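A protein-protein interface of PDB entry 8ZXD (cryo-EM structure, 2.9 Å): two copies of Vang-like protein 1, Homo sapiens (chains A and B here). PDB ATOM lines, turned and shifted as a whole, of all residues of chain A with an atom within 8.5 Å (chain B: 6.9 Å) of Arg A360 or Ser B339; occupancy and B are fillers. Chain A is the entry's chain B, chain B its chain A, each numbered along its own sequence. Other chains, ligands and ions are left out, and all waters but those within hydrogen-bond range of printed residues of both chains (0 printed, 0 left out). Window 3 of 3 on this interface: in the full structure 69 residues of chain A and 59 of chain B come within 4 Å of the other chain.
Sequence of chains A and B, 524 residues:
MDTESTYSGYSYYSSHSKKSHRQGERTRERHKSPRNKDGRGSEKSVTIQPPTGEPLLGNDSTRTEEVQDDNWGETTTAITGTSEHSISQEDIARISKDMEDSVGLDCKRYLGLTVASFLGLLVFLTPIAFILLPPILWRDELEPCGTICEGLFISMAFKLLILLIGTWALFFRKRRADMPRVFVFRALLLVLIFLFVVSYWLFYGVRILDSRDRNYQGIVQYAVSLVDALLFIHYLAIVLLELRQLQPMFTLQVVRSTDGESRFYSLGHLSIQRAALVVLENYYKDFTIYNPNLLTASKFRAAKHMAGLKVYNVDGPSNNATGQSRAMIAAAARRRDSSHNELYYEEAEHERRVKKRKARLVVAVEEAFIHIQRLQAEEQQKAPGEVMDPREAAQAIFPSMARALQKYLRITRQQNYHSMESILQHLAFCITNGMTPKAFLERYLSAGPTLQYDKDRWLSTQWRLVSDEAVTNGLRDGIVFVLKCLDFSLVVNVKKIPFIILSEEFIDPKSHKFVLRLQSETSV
Among the printed residues, pairs that only touch across the chains: Ala A359 with Asn B341 (3.5 Å), Ala A359 with Leu B343 (3.9 Å), Arg A360 with Arg B336 (3.9 Å), Val A362 with Leu B343 (3.97 Å), Val A363 with Arg B336 (3.6 Å), Ala A364 with Arg B336 (3.4 Å) and Arg A403 with Arg B334 (3.5 Å).
No position is printed for both chains.
OG of Ser B339 is in hydrogen-bond range of O of Arg B335 (3.2 Å).
OD1 of Asp B337 lies within salt-bridge range of NE of Arg B336 (3.9 Å).
OE1 of Glu A367 is in salt-bridge range of NH1 of Arg B336 (2.4 Å).
O of Asp B337 is in hydrogen-bond range of NH1 of Arg A360 (2.5 Å).
The side-chain carboxylate (OD2) of Asp B337 is in salt-bridge range of the guanidinium group (NH1) of Arg A403 (3.2 Å).
The backbone carbonyl oxygen (O) of Ser B339 sits at hydrogen-bond distance from the guanidinium group (NH1) of Arg A360 (3.3 Å).
The side-chain amide nitrogen (ND2) of Asn B341 sits at hydrogen-bond distance from the backbone carbonyl oxygen (O) of Lys A356 (3.3 Å).
Of the 23 printed residues of chain A, 8 touch a printed residue of chain B.
Printed residues of chain A that touch a printed residue of chain B: Lys A356, Ala A359, Arg A360, Val A362, Val A363, Ala A364, Glu A367 and Arg A403.
Hydrophobic or aromatic side chains of chain A that line the printed part of chain B: Ala A359, Val A362, Val A363 and Ala A364.
Hydrophobic or aromatic side chains of chain B that line the printed part of chain A: Leu B343.
Among the printed residues, 12 pairs touch across the chains.
Of chain B, only Arg B336, Asp B337 and Ser B339 come within 4 Å of Arg A360.
Printed residues of chain B within 4 Å of Val A363: Arg B336.
Printed residues of chain B within 4 Å of Glu A367: Arg B336 (2.4 Å).
Of the printed residues of chain A, Arg B336 touches Arg A360, Val A363, Ala A364 and Glu A367.
No residue of chain A comes within 4 Å of Ser B338.
Ser B339 touches just one residue of chain A: Arg A360.
The nearest residue of chain A that does not touch Ser B339 is Val A363 (8.3 Å).
The nearest printed residue of chain A that does not touch Asn B341 is Arg A360 (4.2 Å).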
ATOM      1  N   ARG A 353       6.339 -27.389  24.910  1.00  0.00           N
ATOM      2  CA  ARG A 353       5.891 -26.380  25.865  1.00  0.00           C
ATOM      3  C   ARG A 353       5.157 -25.244  25.162  1.00  0.00           C
ATOM      4  O   ARG A 353       4.133 -24.754  25.657  1.00  0.00           O
ATOM      5  CB  ARG A 353       7.082 -25.839  26.656  1.00  0.00           C
ATOM      6  CG  ARG A 353       7.627 -26.799  27.700  1.00  0.00           C
ATOM      7  CD  ARG A 353       9.122 -26.605  27.896  1.00  0.00           C
ATOM      8  NE  ARG A 353       9.746 -27.764  28.525  1.00  0.00           N
ATOM      9  CZ  ARG A 353      11.039 -27.857  28.806  1.00  0.00           C
ATOM     10  NH1 ARG A 353      11.880 -26.875  28.525  1.00  0.00           N
ATOM     11  NH2 ARG A 353      11.500 -28.963  29.383  1.00  0.00           N
ATOM     12  N   VAL A 354       5.668 -24.813  24.006  1.00  0.00           N
ATOM     13  CA  VAL A 354       5.017 -23.748  23.248  1.00  0.00           C
ATOM     14  C   VAL A 354       3.631 -24.187  22.797  1.00  0.00           C
ATOM     15  O   VAL A 354       2.669 -23.416  22.873  1.00  0.00           O
ATOM     16  CB  VAL A 354       5.897 -23.324  22.057  1.00  0.00           C
ATOM     17  CG1 VAL A 354       5.098 -22.484  21.072  1.00  0.00           C
ATOM     18  CG2 VAL A 354       7.109 -22.547  22.547  1.00  0.00           C
ATOM     19  N   LYS A 355       3.503 -25.427  22.321  1.00  0.00           N
ATOM     20  CA  LYS A 355       2.199 -25.927  21.897  1.00  0.00           C
ATOM     21  C   LYS A 355       1.222 -25.997  23.067  1.00  0.00           C
ATOM     22  O   LYS A 355       0.048 -25.628  22.930  1.00  0.00           O
ATOM     23  CB  LYS A 355       2.348 -27.300  21.241  1.00  0.00           C
ATOM     24  CG  LYS A 355       3.005 -27.265  19.871  1.00  0.00           C
ATOM     25  CD  LYS A 355       3.088 -28.655  19.263  1.00  0.00           C
ATOM     26  CE  LYS A 355       3.888 -28.647  17.971  1.00  0.00           C
ATOM     27  NZ  LYS A 355       3.209 -27.864  16.902  1.00  0.00           N
ATOM     28  N   LYS A 356       1.685 -26.476  24.225  1.00  0.00           N
ATOM     29  CA  LYS A 356       0.810 -26.562  25.392  1.00  0.00           C
ATOM     30  C   LYS A 356       0.344 -25.180  25.833  1.00  0.00           C
ATOM     31  O   LYS A 356      -0.843 -24.970  26.120  1.00  0.00           O
ATOM     32  CB  LYS A 356       1.529 -27.281  26.534  1.00  0.00           C
ATOM     33  CG  LYS A 356       1.729 -28.770  26.304  1.00  0.00           C
ATOM     34  CD  LYS A 356       2.415 -29.424  27.492  1.00  0.00           C
ATOM     35  CE  LYS A 356       2.641 -30.908  27.250  1.00  0.00           C
ATOM     36  NZ  LYS A 356       3.335 -31.557  28.396  1.00  0.00           N
ATOM     37  N   ARG A 357       1.267 -24.216  25.885  1.00  0.00           N
ATOM     38  CA  ARG A 357       0.889 -22.863  26.276  1.00  0.00           C
ATOM     39  C   ARG A 357      -0.008 -22.209  25.232  1.00  0.00           C
ATOM     40  O   ARG A 357      -0.892 -21.424  25.587  1.00  0.00           O
ATOM     41  CB  ARG A 357       2.137 -22.018  26.526  1.00  0.00           C
ATOM     42  CG  ARG A 357       2.958 -22.491  27.717  1.00  0.00           C
ATOM     43  CD  ARG A 357       4.137 -21.575  27.982  1.00  0.00           C
ATOM     44  NE  ARG A 357       4.697 -21.774  29.314  1.00  0.00           N
ATOM     45  CZ  ARG A 357       5.332 -20.840  30.006  1.00  0.00           C
ATOM     46  NH1 ARG A 357       5.511 -19.621  29.522  1.00  0.00           N
ATOM     47  NH2 ARG A 357       5.802 -21.134  31.216  1.00  0.00           N
ATOM     48  N   LYS A 358       0.194 -22.524  23.951  1.00  0.00           N
ATOM     49  CA  LYS A 358      -0.698 -22.026  22.910  1.00  0.00           C
ATOM     50  C   LYS A 358      -2.109 -22.565  23.093  1.00  0.00           C
ATOM     51  O   LYS A 358      -3.086 -21.822  22.955  1.00  0.00           O
ATOM     52  CB  LYS A 358      -0.153 -22.407  21.534  1.00  0.00           C
ATOM     53  CG  LYS A 358      -1.111 -22.139  20.386  1.00  0.00           C
ATOM     54  CD  LYS A 358      -0.549 -22.655  19.071  1.00  0.00           C
ATOM     55  CE  LYS A 358      -0.539 -24.175  19.033  1.00  0.00           C
ATOM     56  NZ  LYS A 358      -1.916 -24.739  19.000  1.00  0.00           N
ATOM     57  N   ALA A 359      -2.235 -23.858  23.402  1.00  0.00           N
ATOM     58  CA  ALA A 359      -3.556 -24.428  23.650  1.00  0.00           C
ATOM     59  C   ALA A 359      -4.214 -23.787  24.866  1.00  0.00           C
ATOM     60  O   ALA A 359      -5.412 -23.472  24.844  1.00  0.00           O
ATOM     61  CB  ALA A 359      -3.449 -25.942  23.831  1.00  0.00           C
ATOM     62  N   ARG A 360      -3.442 -23.581  25.938  1.00  0.00           N
ATOM     63  CA  ARG A 360      -3.990 -22.935  27.127  1.00  0.00           C
ATOM     64  C   ARG A 360      -4.442 -21.510  26.824  1.00  0.00           C
ATOM     65  O   ARG A 360      -5.504 -21.075  27.284  1.00  0.00           O
ATOM     66  CB  ARG A 360      -2.958 -22.945  28.254  1.00  0.00           C
ATOM     67  CG  ARG A 360      -2.645 -24.331  28.793  1.00  0.00           C
ATOM     68  CD  ARG A 360      -1.728 -24.262  30.003  1.00  0.00           C
ATOM     69  NE  ARG A 360      -1.319 -25.587  30.454  1.00  0.00           N
ATOM     70  CZ  ARG A 360      -2.024 -26.348  31.278  1.00  0.00           C
ATOM     71  NH1 ARG A 360      -3.187 -25.948  31.766  1.00  0.00           N
ATOM     72  NH2 ARG A 360      -1.551 -27.543  31.622  1.00  0.00           N
ATOM     73  N   LEU A 361      -3.646 -20.771  26.046  1.00  0.00           N
ATOM     74  CA  LEU A 361      -4.019 -19.411  25.672  1.00  0.00           C
ATOM     75  C   LEU A 361      -5.266 -19.402  24.798  1.00  0.00           C
ATOM     76  O   LEU A 361      -6.115 -18.514  24.928  1.00  0.00           O
ATOM     77  CB  LEU A 361      -2.854 -18.727  24.957  1.00  0.00           C
ATOM     78  CG  LEU A 361      -3.094 -17.297  24.468  1.00  0.00           C
ATOM     79  CD1 LEU A 361      -3.469 -16.388  25.628  1.00  0.00           C
ATOM     80  CD2 LEU A 361      -1.870 -16.767  23.737  1.00  0.00           C
ATOM     81  N   VAL A 362      -5.390 -20.376  23.894  1.00  0.00           N
ATOM     82  CA  VAL A 362      -6.581 -20.468  23.052  1.00  0.00           C
ATOM     83  C   VAL A 362      -7.817 -20.704  23.911  1.00  0.00           C
ATOM     84  O   VAL A 362      -8.863 -20.072  23.714  1.00  0.00           O
ATOM     85  CB  VAL A 362      -6.406 -21.574  21.994  1.00  0.00           C
ATOM     86  CG1 VAL A 362      -7.750 -21.952  21.387  1.00  0.00           C
ATOM     87  CG2 VAL A 362      -5.438 -21.125  20.910  1.00  0.00           C
ATOM     88  N   VAL A 363      -7.712 -21.615  24.882  1.00  0.00           N
ATOM     89  CA  VAL A 363      -8.842 -21.884  25.771  1.00  0.00           C
ATOM     90  C   VAL A 363      -9.195 -20.638  26.578  1.00  0.00           C
ATOM     91  O   VAL A 363     -10.376 -20.295  26.739  1.00  0.00           O
ATOM     92  CB  VAL A 363      -8.529 -23.083  26.686  1.00  0.00           C
ATOM     93  CG1 VAL A 363      -9.625 -23.261  27.725  1.00  0.00           C
ATOM     94  CG2 VAL A 363      -8.367 -24.350  25.859  1.00  0.00           C
ATOM     95  N   ALA A 364      -8.180 -19.942  27.096  1.00  0.00           N
ATOM     96  CA  ALA A 364      -8.429 -18.735  27.879  1.00  0.00           C
ATOM     97  C   ALA A 364      -9.093 -17.653  27.037  1.00  0.00           C
ATOM     98  O   ALA A 364     -10.008 -16.966  27.505  1.00  0.00           O
ATOM     99  CB  ALA A 364      -7.122 -18.220  28.481  1.00  0.00           C
ATOM    100  N   VAL A 365      -8.648 -17.487  25.790  1.00  0.00           N
ATOM    101  CA  VAL A 365      -9.229 -16.471  24.918  1.00  0.00           C
ATOM    102  C   VAL A 365     -10.662 -16.835  24.551  1.00  0.00           C
ATOM    103  O   VAL A 365     -11.535 -15.963  24.464  1.00  0.00           O
ATOM    104  CB  VAL A 365      -8.345 -16.274  23.672  1.00  0.00           C
ATOM    105  CG1 VAL A 365      -9.094 -15.512  22.589  1.00  0.00           C
ATOM    106  CG2 VAL A 365      -7.066 -15.541  24.046  1.00  0.00           C
ATOM    107  N   GLU A 366     -10.933 -18.125  24.336  1.00  0.00           N
ATOM    108  CA  GLU A 366     -12.305 -18.549  24.068  1.00  0.00           C
ATOM    109  C   GLU A 366     -13.211 -18.262  25.260  1.00  0.00           C
ATOM    110  O   GLU A 366     -14.335 -17.772  25.093  1.00  0.00           O
ATOM    111  CB  GLU A 366     -12.338 -20.035  23.712  1.00  0.00           C
ATOM    112  CG  GLU A 366     -11.813 -20.350  22.320  1.00  0.00           C
ATOM    113  CD  GLU A 366     -11.908 -21.825  21.982  1.00  0.00           C
ATOM    114  OE1 GLU A 366     -12.252 -22.621  22.880  1.00  0.00           O
ATOM    115  OE2 GLU A 366     -11.641 -22.187  20.817  1.00  0.00           O
ATOM    116  N   GLU A 367     -12.735 -18.552  26.475  1.00  0.00           N
ATOM    117  CA  GLU A 367     -13.524 -18.246  27.665  1.00  0.00           C
ATOM    118  C   GLU A 367     -13.736 -16.743  27.814  1.00  0.00           C
ATOM    119  O   GLU A 367     -14.825 -16.293  28.196  1.00  0.00           O
ATOM    120  CB  GLU A 367     -12.848 -18.821  28.909  1.00  0.00           C
ATOM    121  CG  GLU A 367     -13.617 -18.583  30.199  1.00  0.00           C
ATOM    122  CD  GLU A 367     -12.804 -18.913  31.434  1.00  0.00           C
ATOM    123  OE1 GLU A 367     -12.116 -19.955  31.433  1.00  0.00           O
ATOM    124  OE2 GLU A 367     -12.851 -18.130  32.407  1.00  0.00           O
ATOM    125  N   SER A 400      -8.598 -11.977  32.893  1.00  0.00           N
ATOM    126  CA  SER A 400      -8.919 -13.394  32.741  1.00  0.00           C
ATOM    127  C   SER A 400      -7.873 -14.117  31.901  1.00  0.00           C
ATOM    128  O   SER A 400      -7.442 -15.223  32.250  1.00  0.00           O
ATOM    129  CB  SER A 400     -10.307 -13.552  32.120  1.00  0.00           C
ATOM    130  OG  SER A 400     -10.330 -13.066  30.789  1.00  0.00           O
ATOM    131  N   MET A 401      -7.452 -13.513  30.792  1.00  0.00           N
ATOM    132  CA  MET A 401      -6.461 -14.103  29.902  1.00  0.00           C
ATOM    133  C   MET A 401      -5.068 -13.515  30.086  1.00  0.00           C
ATOM    134  O   MET A 401      -4.157 -13.871  29.329  1.00  0.00           O
ATOM    135  CB  MET A 401      -6.899 -13.936  28.443  1.00  0.00           C
ATOM    136  CG  MET A 401      -6.656 -12.542  27.879  1.00  0.00           C
ATOM    137  SD  MET A 401      -6.755 -12.474  26.080  1.00  0.00           S
ATOM    138  CE  MET A 401      -8.520 -12.294  25.840  1.00  0.00           C
ATOM    139  N   ARG A 403      -2.735 -13.829  32.463  1.00  0.00           N
ATOM    140  CA  ARG A 403      -1.693 -14.773  32.860  1.00  0.00           C
ATOM    141  C   ARG A 403      -1.288 -15.667  31.694  1.00  0.00           C
ATOM    142  O   ARG A 403      -0.096 -15.888  31.450  1.00  0.00           O
ATOM    143  CB  ARG A 403      -2.173 -15.613  34.045  1.00  0.00           C
ATOM    144  CG  ARG A 403      -1.094 -16.487  34.663  1.00  0.00           C
ATOM    145  CD  ARG A 403      -1.610 -17.207  35.898  1.00  0.00           C
ATOM    146  NE  ARG A 403      -0.555 -17.952  36.575  1.00  0.00           N
ATOM    147  CZ  ARG A 403      -0.237 -19.211  36.308  1.00  0.00           C
ATOM    148  NH1 ARG A 403      -0.876 -19.902  35.378  1.00  0.00           N
ATOM    149  NH2 ARG A 403       0.746 -19.792  36.989  1.00  0.00           N
ATOM    150  N   ALA A 404      -2.274 -16.188  30.959  1.00  0.00           N
ATOM    151  CA  ALA A 404      -1.972 -17.043  29.816  1.00  0.00           C
ATOM    152  C   ALA A 404      -1.217 -16.278  28.737  1.00  0.00           C
ATOM    153  O   ALA A 404      -0.255 -16.796  28.155  1.00  0.00           O
ATOM    154  CB  ALA A 404      -3.262 -17.638  29.251  1.00  0.00           C
ATOM    155  N   LEU A 405      -1.635 -15.041  28.457  1.00  0.00           N
ATOM    156  CA  LEU A 405      -0.953 -14.246  27.441  1.00  0.00           C
ATOM    157  C   LEU A 405       0.476 -13.922  27.859  1.00  0.00           C
ATOM    158  O   LEU A 405       1.394 -13.972  27.032  1.00  0.00           O
ATOM    159  CB  LEU A 405      -1.741 -12.967  27.162  1.00  0.00           C
ATOM    160  CG  LEU A 405      -1.384 -12.221  25.876  1.00  0.00           C
ATOM    161  CD1 LEU A 405      -1.568 -13.124  24.667  1.00  0.00           C
ATOM    162  CD2 LEU A 405      -2.238 -10.973  25.741  1.00  0.00           C
ATOM    163  N   LYS A 407       2.366 -15.724  29.889  1.00  0.00           N
ATOM    164  CA  LYS A 407       3.135 -16.962  29.782  1.00  0.00           C
ATOM    165  C   LYS A 407       3.501 -17.260  28.334  1.00  0.00           C
ATOM    166  O   LYS A 407       4.633 -17.668  28.041  1.00  0.00           O
ATOM    167  CB  LYS A 407       2.348 -18.122  30.391  1.00  0.00           C
ATOM    168  CG  LYS A 407       2.277 -18.095  31.909  1.00  0.00           C
ATOM    169  CD  LYS A 407       1.651 -19.368  32.456  1.00  0.00           C
ATOM    170  CE  LYS A 407       2.495 -20.587  32.121  1.00  0.00           C
ATOM    171  NZ  LYS A 407       1.885 -21.843  32.637  1.00  0.00           N
ATOM    172  N   TYR A 408       2.555 -17.065  27.410  1.00  0.00           N
ATOM    173  CA  TYR A 408       2.843 -17.305  26.000  1.00  0.00           C
ATOM    174  C   TYR A 408       3.894 -16.334  25.476  1.00  0.00           C
ATOM    175  O   TYR A 408       4.778 -16.725  24.705  1.00  0.00           O
ATOM    176  CB  TYR A 408       1.562 -17.208  25.173  1.00  0.00           C
ATOM    177  CG  TYR A 408       1.733 -17.678  23.747  1.00  0.00           C
ATOM    178  CD1 TYR A 408       1.907 -19.025  23.456  1.00  0.00           C
ATOM    179  CD2 TYR A 408       1.728 -16.776  22.692  1.00  0.00           C
ATOM    180  CE1 TYR A 408       2.066 -19.461  22.156  1.00  0.00           C
ATOM    181  CE2 TYR A 408       1.886 -17.203  21.387  1.00  0.00           C
ATOM    182  CZ  TYR A 408       2.056 -18.546  21.125  1.00  0.00           C
ATOM    183  OH  TYR A 408       2.215 -18.976  19.828  1.00  0.00           O
ATOM    184  N   LEU A 441      -6.114 -14.248  18.496  1.00  0.00           N
ATOM    185  CA  LEU A 441      -5.009 -15.115  18.894  1.00  0.00           C
ATOM    186  C   LEU A 441      -3.856 -15.055  17.899  1.00  0.00           C
ATOM    187  O   LEU A 441      -2.686 -15.032  18.299  1.00  0.00           O
ATOM    188  CB  LEU A 441      -5.507 -16.552  19.046  1.00  0.00           C
ATOM    189  CG  LEU A 441      -6.214 -16.890  20.358  1.00  0.00           C
ATOM    190  CD1 LEU A 441      -7.200 -18.028  20.157  1.00  0.00           C
ATOM    191  CD2 LEU A 441      -5.193 -17.250  21.423  1.00  0.00           C
ATOM    192  N   ALA B 332     -10.553 -18.418  39.150  1.00  0.00           N
ATOM    193  CA  ALA B 332     -11.036 -19.442  38.228  1.00  0.00           C
ATOM    194  C   ALA B 332     -10.049 -19.671  37.091  1.00  0.00           C
ATOM    195  O   ALA B 332      -9.789 -20.817  36.706  1.00  0.00           O
ATOM    196  CB  ALA B 332     -12.407 -19.049  37.680  1.00  0.00           C
ATOM    197  N   ARG B 334      -6.802 -19.093  37.204  1.00  0.00           N
ATOM    198  CA  ARG B 334      -5.633 -19.752  37.778  1.00  0.00           C
ATOM    199  C   ARG B 334      -5.882 -21.242  37.977  1.00  0.00           C
ATOM    200  O   ARG B 334      -4.999 -22.068  37.714  1.00  0.00           O
ATOM    201  CB  ARG B 334      -5.254 -19.089  39.102  1.00  0.00           C
ATOM    202  CG  ARG B 334      -4.477 -17.792  38.948  1.00  0.00           C
ATOM    203  CD  ARG B 334      -3.970 -17.290  40.290  1.00  0.00           C
ATOM    204  NE  ARG B 334      -2.997 -16.215  40.139  1.00  0.00           N
ATOM    205  CZ  ARG B 334      -1.690 -16.399  40.010  1.00  0.00           C
ATOM    206  NH1 ARG B 334      -1.160 -17.611  40.009  1.00  0.00           N
ATOM    207  NH2 ARG B 334      -0.895 -15.341  39.879  1.00  0.00           N
ATOM    208  N   ARG B 335      -7.078 -21.605  38.449  1.00  0.00           N
ATOM    209  CA  ARG B 335      -7.416 -23.016  38.605  1.00  0.00           C
ATOM    210  C   ARG B 335      -7.473 -23.721  37.255  1.00  0.00           C
ATOM    211  O   ARG B 335      -7.042 -24.874  37.128  1.00  0.00           O
ATOM    212  CB  ARG B 335      -8.745 -23.160  39.345  1.00  0.00           C
ATOM    213  CG  ARG B 335      -8.660 -22.868  40.834  1.00  0.00           C
ATOM    214  CD  ARG B 335      -9.953 -23.233  41.545  1.00  0.00           C
ATOM    215  NE  ARG B 335     -10.945 -22.167  41.458  1.00  0.00           N
ATOM    216  CZ  ARG B 335     -12.026 -22.210  40.691  1.00  0.00           C
ATOM    217  NH1 ARG B 335     -12.289 -23.258  39.927  1.00  0.00           N
ATOM    218  NH2 ARG B 335     -12.862 -21.177  40.691  1.00  0.00           N
ATOM    219  N   ARG B 336      -8.009 -23.046  36.236  1.00  0.00           N
ATOM    220  CA  ARG B 336      -8.076 -23.634  34.901  1.00  0.00           C
ATOM    221  C   ARG B 336      -6.683 -23.853  34.323  1.00  0.00           C
ATOM    222  O   ARG B 336      -6.448 -24.838  33.614  1.00  0.00           O
ATOM    223  CB  ARG B 336      -8.909 -22.743  33.980  1.00  0.00           C
ATOM    224  CG  ARG B 336      -9.185 -23.337  32.605  1.00  0.00           C
ATOM    225  CD  ARG B 336      -8.263 -22.747  31.547  1.00  0.00           C
ATOM    226  NE  ARG B 336      -8.198 -21.293  31.627  1.00  0.00           N
ATOM    227  CZ  ARG B 336      -9.097 -20.472  31.100  1.00  0.00           C
ATOM    228  NH1 ARG B 336     -10.147 -20.929  30.437  1.00  0.00           N
ATOM    229  NH2 ARG B 336      -8.938 -19.159  31.242  1.00  0.00           N
ATOM    230  N   ASP B 337      -5.751 -22.938  34.606  1.00  0.00           N
ATOM    231  CA  ASP B 337      -4.394 -23.076  34.084  1.00  0.00           C
ATOM    232  C   ASP B 337      -3.711 -24.332  34.609  1.00  0.00           C
ATOM    233  O   ASP B 337      -2.820 -24.875  33.947  1.00  0.00           O
ATOM    234  CB  ASP B 337      -3.570 -21.836  34.434  1.00  0.00           C
ATOM    235  CG  ASP B 337      -3.963 -20.623  33.614  1.00  0.00           C
ATOM    236  OD1 ASP B 337      -4.424 -20.804  32.467  1.00  0.00           O
ATOM    237  OD2 ASP B 337      -3.811 -19.491  34.116  1.00  0.00           O
ATOM    238  N   SER B 338      -4.108 -24.805  35.787  1.00  0.00           N
ATOM    239  CA  SER B 338      -3.559 -26.025  36.363  1.00  0.00           C
ATOM    240  C   SER B 338      -4.350 -27.269  35.978  1.00  0.00           C
ATOM    241  O   SER B 338      -3.987 -28.372  36.402  1.00  0.00           O
ATOM    242  CB  SER B 338      -3.498 -25.906  37.889  1.00  0.00           C
ATOM    243  OG  SER B 338      -4.798 -25.824  38.448  1.00  0.00           O
ATOM    244  N   SER B 339      -5.414 -27.123  35.194  1.00  0.00           N
ATOM    245  CA  SER B 339      -6.238 -28.255  34.799  1.00  0.00           C
ATOM    246  C   SER B 339      -5.594 -28.999  33.631  1.00  0.00           C
ATOM    247  O   SER B 339      -4.529 -28.631  33.128  1.00  0.00           O
ATOM    248  CB  SER B 339      -7.648 -27.785  34.445  1.00  0.00           C
ATOM    249  OG  SER B 339      -8.367 -27.409  35.606  1.00  0.00           O
ATOM    250  N   HIS B 340      -6.255 -30.068  33.195  1.00  0.00           N
ATOM    251  CA  HIS B 340      -5.739 -30.879  32.100  1.00  0.00           C
ATOM    252  C   HIS B 340      -5.803 -30.115  30.784  1.00  0.00           C
ATOM    253  O   HIS B 340      -6.759 -29.384  30.514  1.00  0.00           O
ATOM    254  CB  HIS B 340      -6.532 -32.181  31.987  1.00  0.00           C
ATOM    255  CG  HIS B 340      -5.883 -33.211  31.117  1.00  0.00           C
ATOM    256  ND1 HIS B 340      -6.548 -33.844  30.089  1.00  0.00           N
ATOM    257  CD2 HIS B 340      -4.629 -33.722  31.125  1.00  0.00           C
ATOM    258  CE1 HIS B 340      -5.732 -34.700  29.500  1.00  0.00           C
ATOM    259  NE2 HIS B 340      -4.561 -34.645  30.110  1.00  0.00           N
ATOM    260  N   ASN B 341      -4.770 -30.290  29.957  1.00  0.00           N
ATOM    261  CA  ASN B 341      -4.710 -29.664  28.637  1.00  0.00           C
ATOM    262  C   ASN B 341      -5.349 -30.613  27.626  1.00  0.00           C
ATOM    263  O   ASN B 341      -4.683 -31.379  26.926  1.00  0.00           O
ATOM    264  CB  ASN B 341      -3.272 -29.322  28.267  1.00  0.00           C
ATOM    265  CG  ASN B 341      -3.184 -28.348  27.110  1.00  0.00           C
ATOM    266  OD1 ASN B 341      -4.201 -27.912  26.569  1.00  0.00           O
ATOM    267  ND2 ASN B 341      -1.964 -27.999  26.723  1.00  0.00           N
ATOM    268  N   GLU B 342      -6.681 -30.551  27.553  1.00  0.00           N
ATOM    269  CA  GLU B 342      -7.423 -31.442  26.668  1.00  0.00           C
ATOM    270  C   GLU B 342      -7.180 -31.122  25.198  1.00  0.00           C
ATOM    271  O   GLU B 342      -7.185 -32.031  24.359  1.00  0.00           O
ATOM    272  CB  GLU B 342      -8.917 -31.367  26.983  1.00  0.00           C
ATOM    273  CG  GLU B 342      -9.734 -32.513  26.413  1.00  0.00           C
ATOM    274  CD  GLU B 342     -11.222 -32.218  26.402  1.00  0.00           C
ATOM    275  OE1 GLU B 342     -11.609 -31.126  25.934  1.00  0.00           O
ATOM    276  OE2 GLU B 342     -12.003 -33.079  26.859  1.00  0.00           O
ATOM    277  N   LEU B 343      -6.972 -29.845  24.867  1.00  0.00           N
ATOM    278  CA  LEU B 343      -6.852 -29.446  23.468  1.00  0.00           C
ATOM    279  C   LEU B 343      -5.615 -30.049  22.809  1.00  0.00           C
ATOM    280  O   LEU B 343      -5.677 -30.493  21.656  1.00  0.00           O
ATOM    281  CB  LEU B 343      -6.824 -27.922  23.362  1.00  0.00           C
ATOM    282  CG  LEU B 343      -6.945 -27.319  21.960  1.00  0.00           C
ATOM    283  CD1 LEU B 343      -8.117 -27.925  21.207  1.00  0.00           C
ATOM    284  CD2 LEU B 343      -7.076 -25.806  22.036  1.00  0.00           C
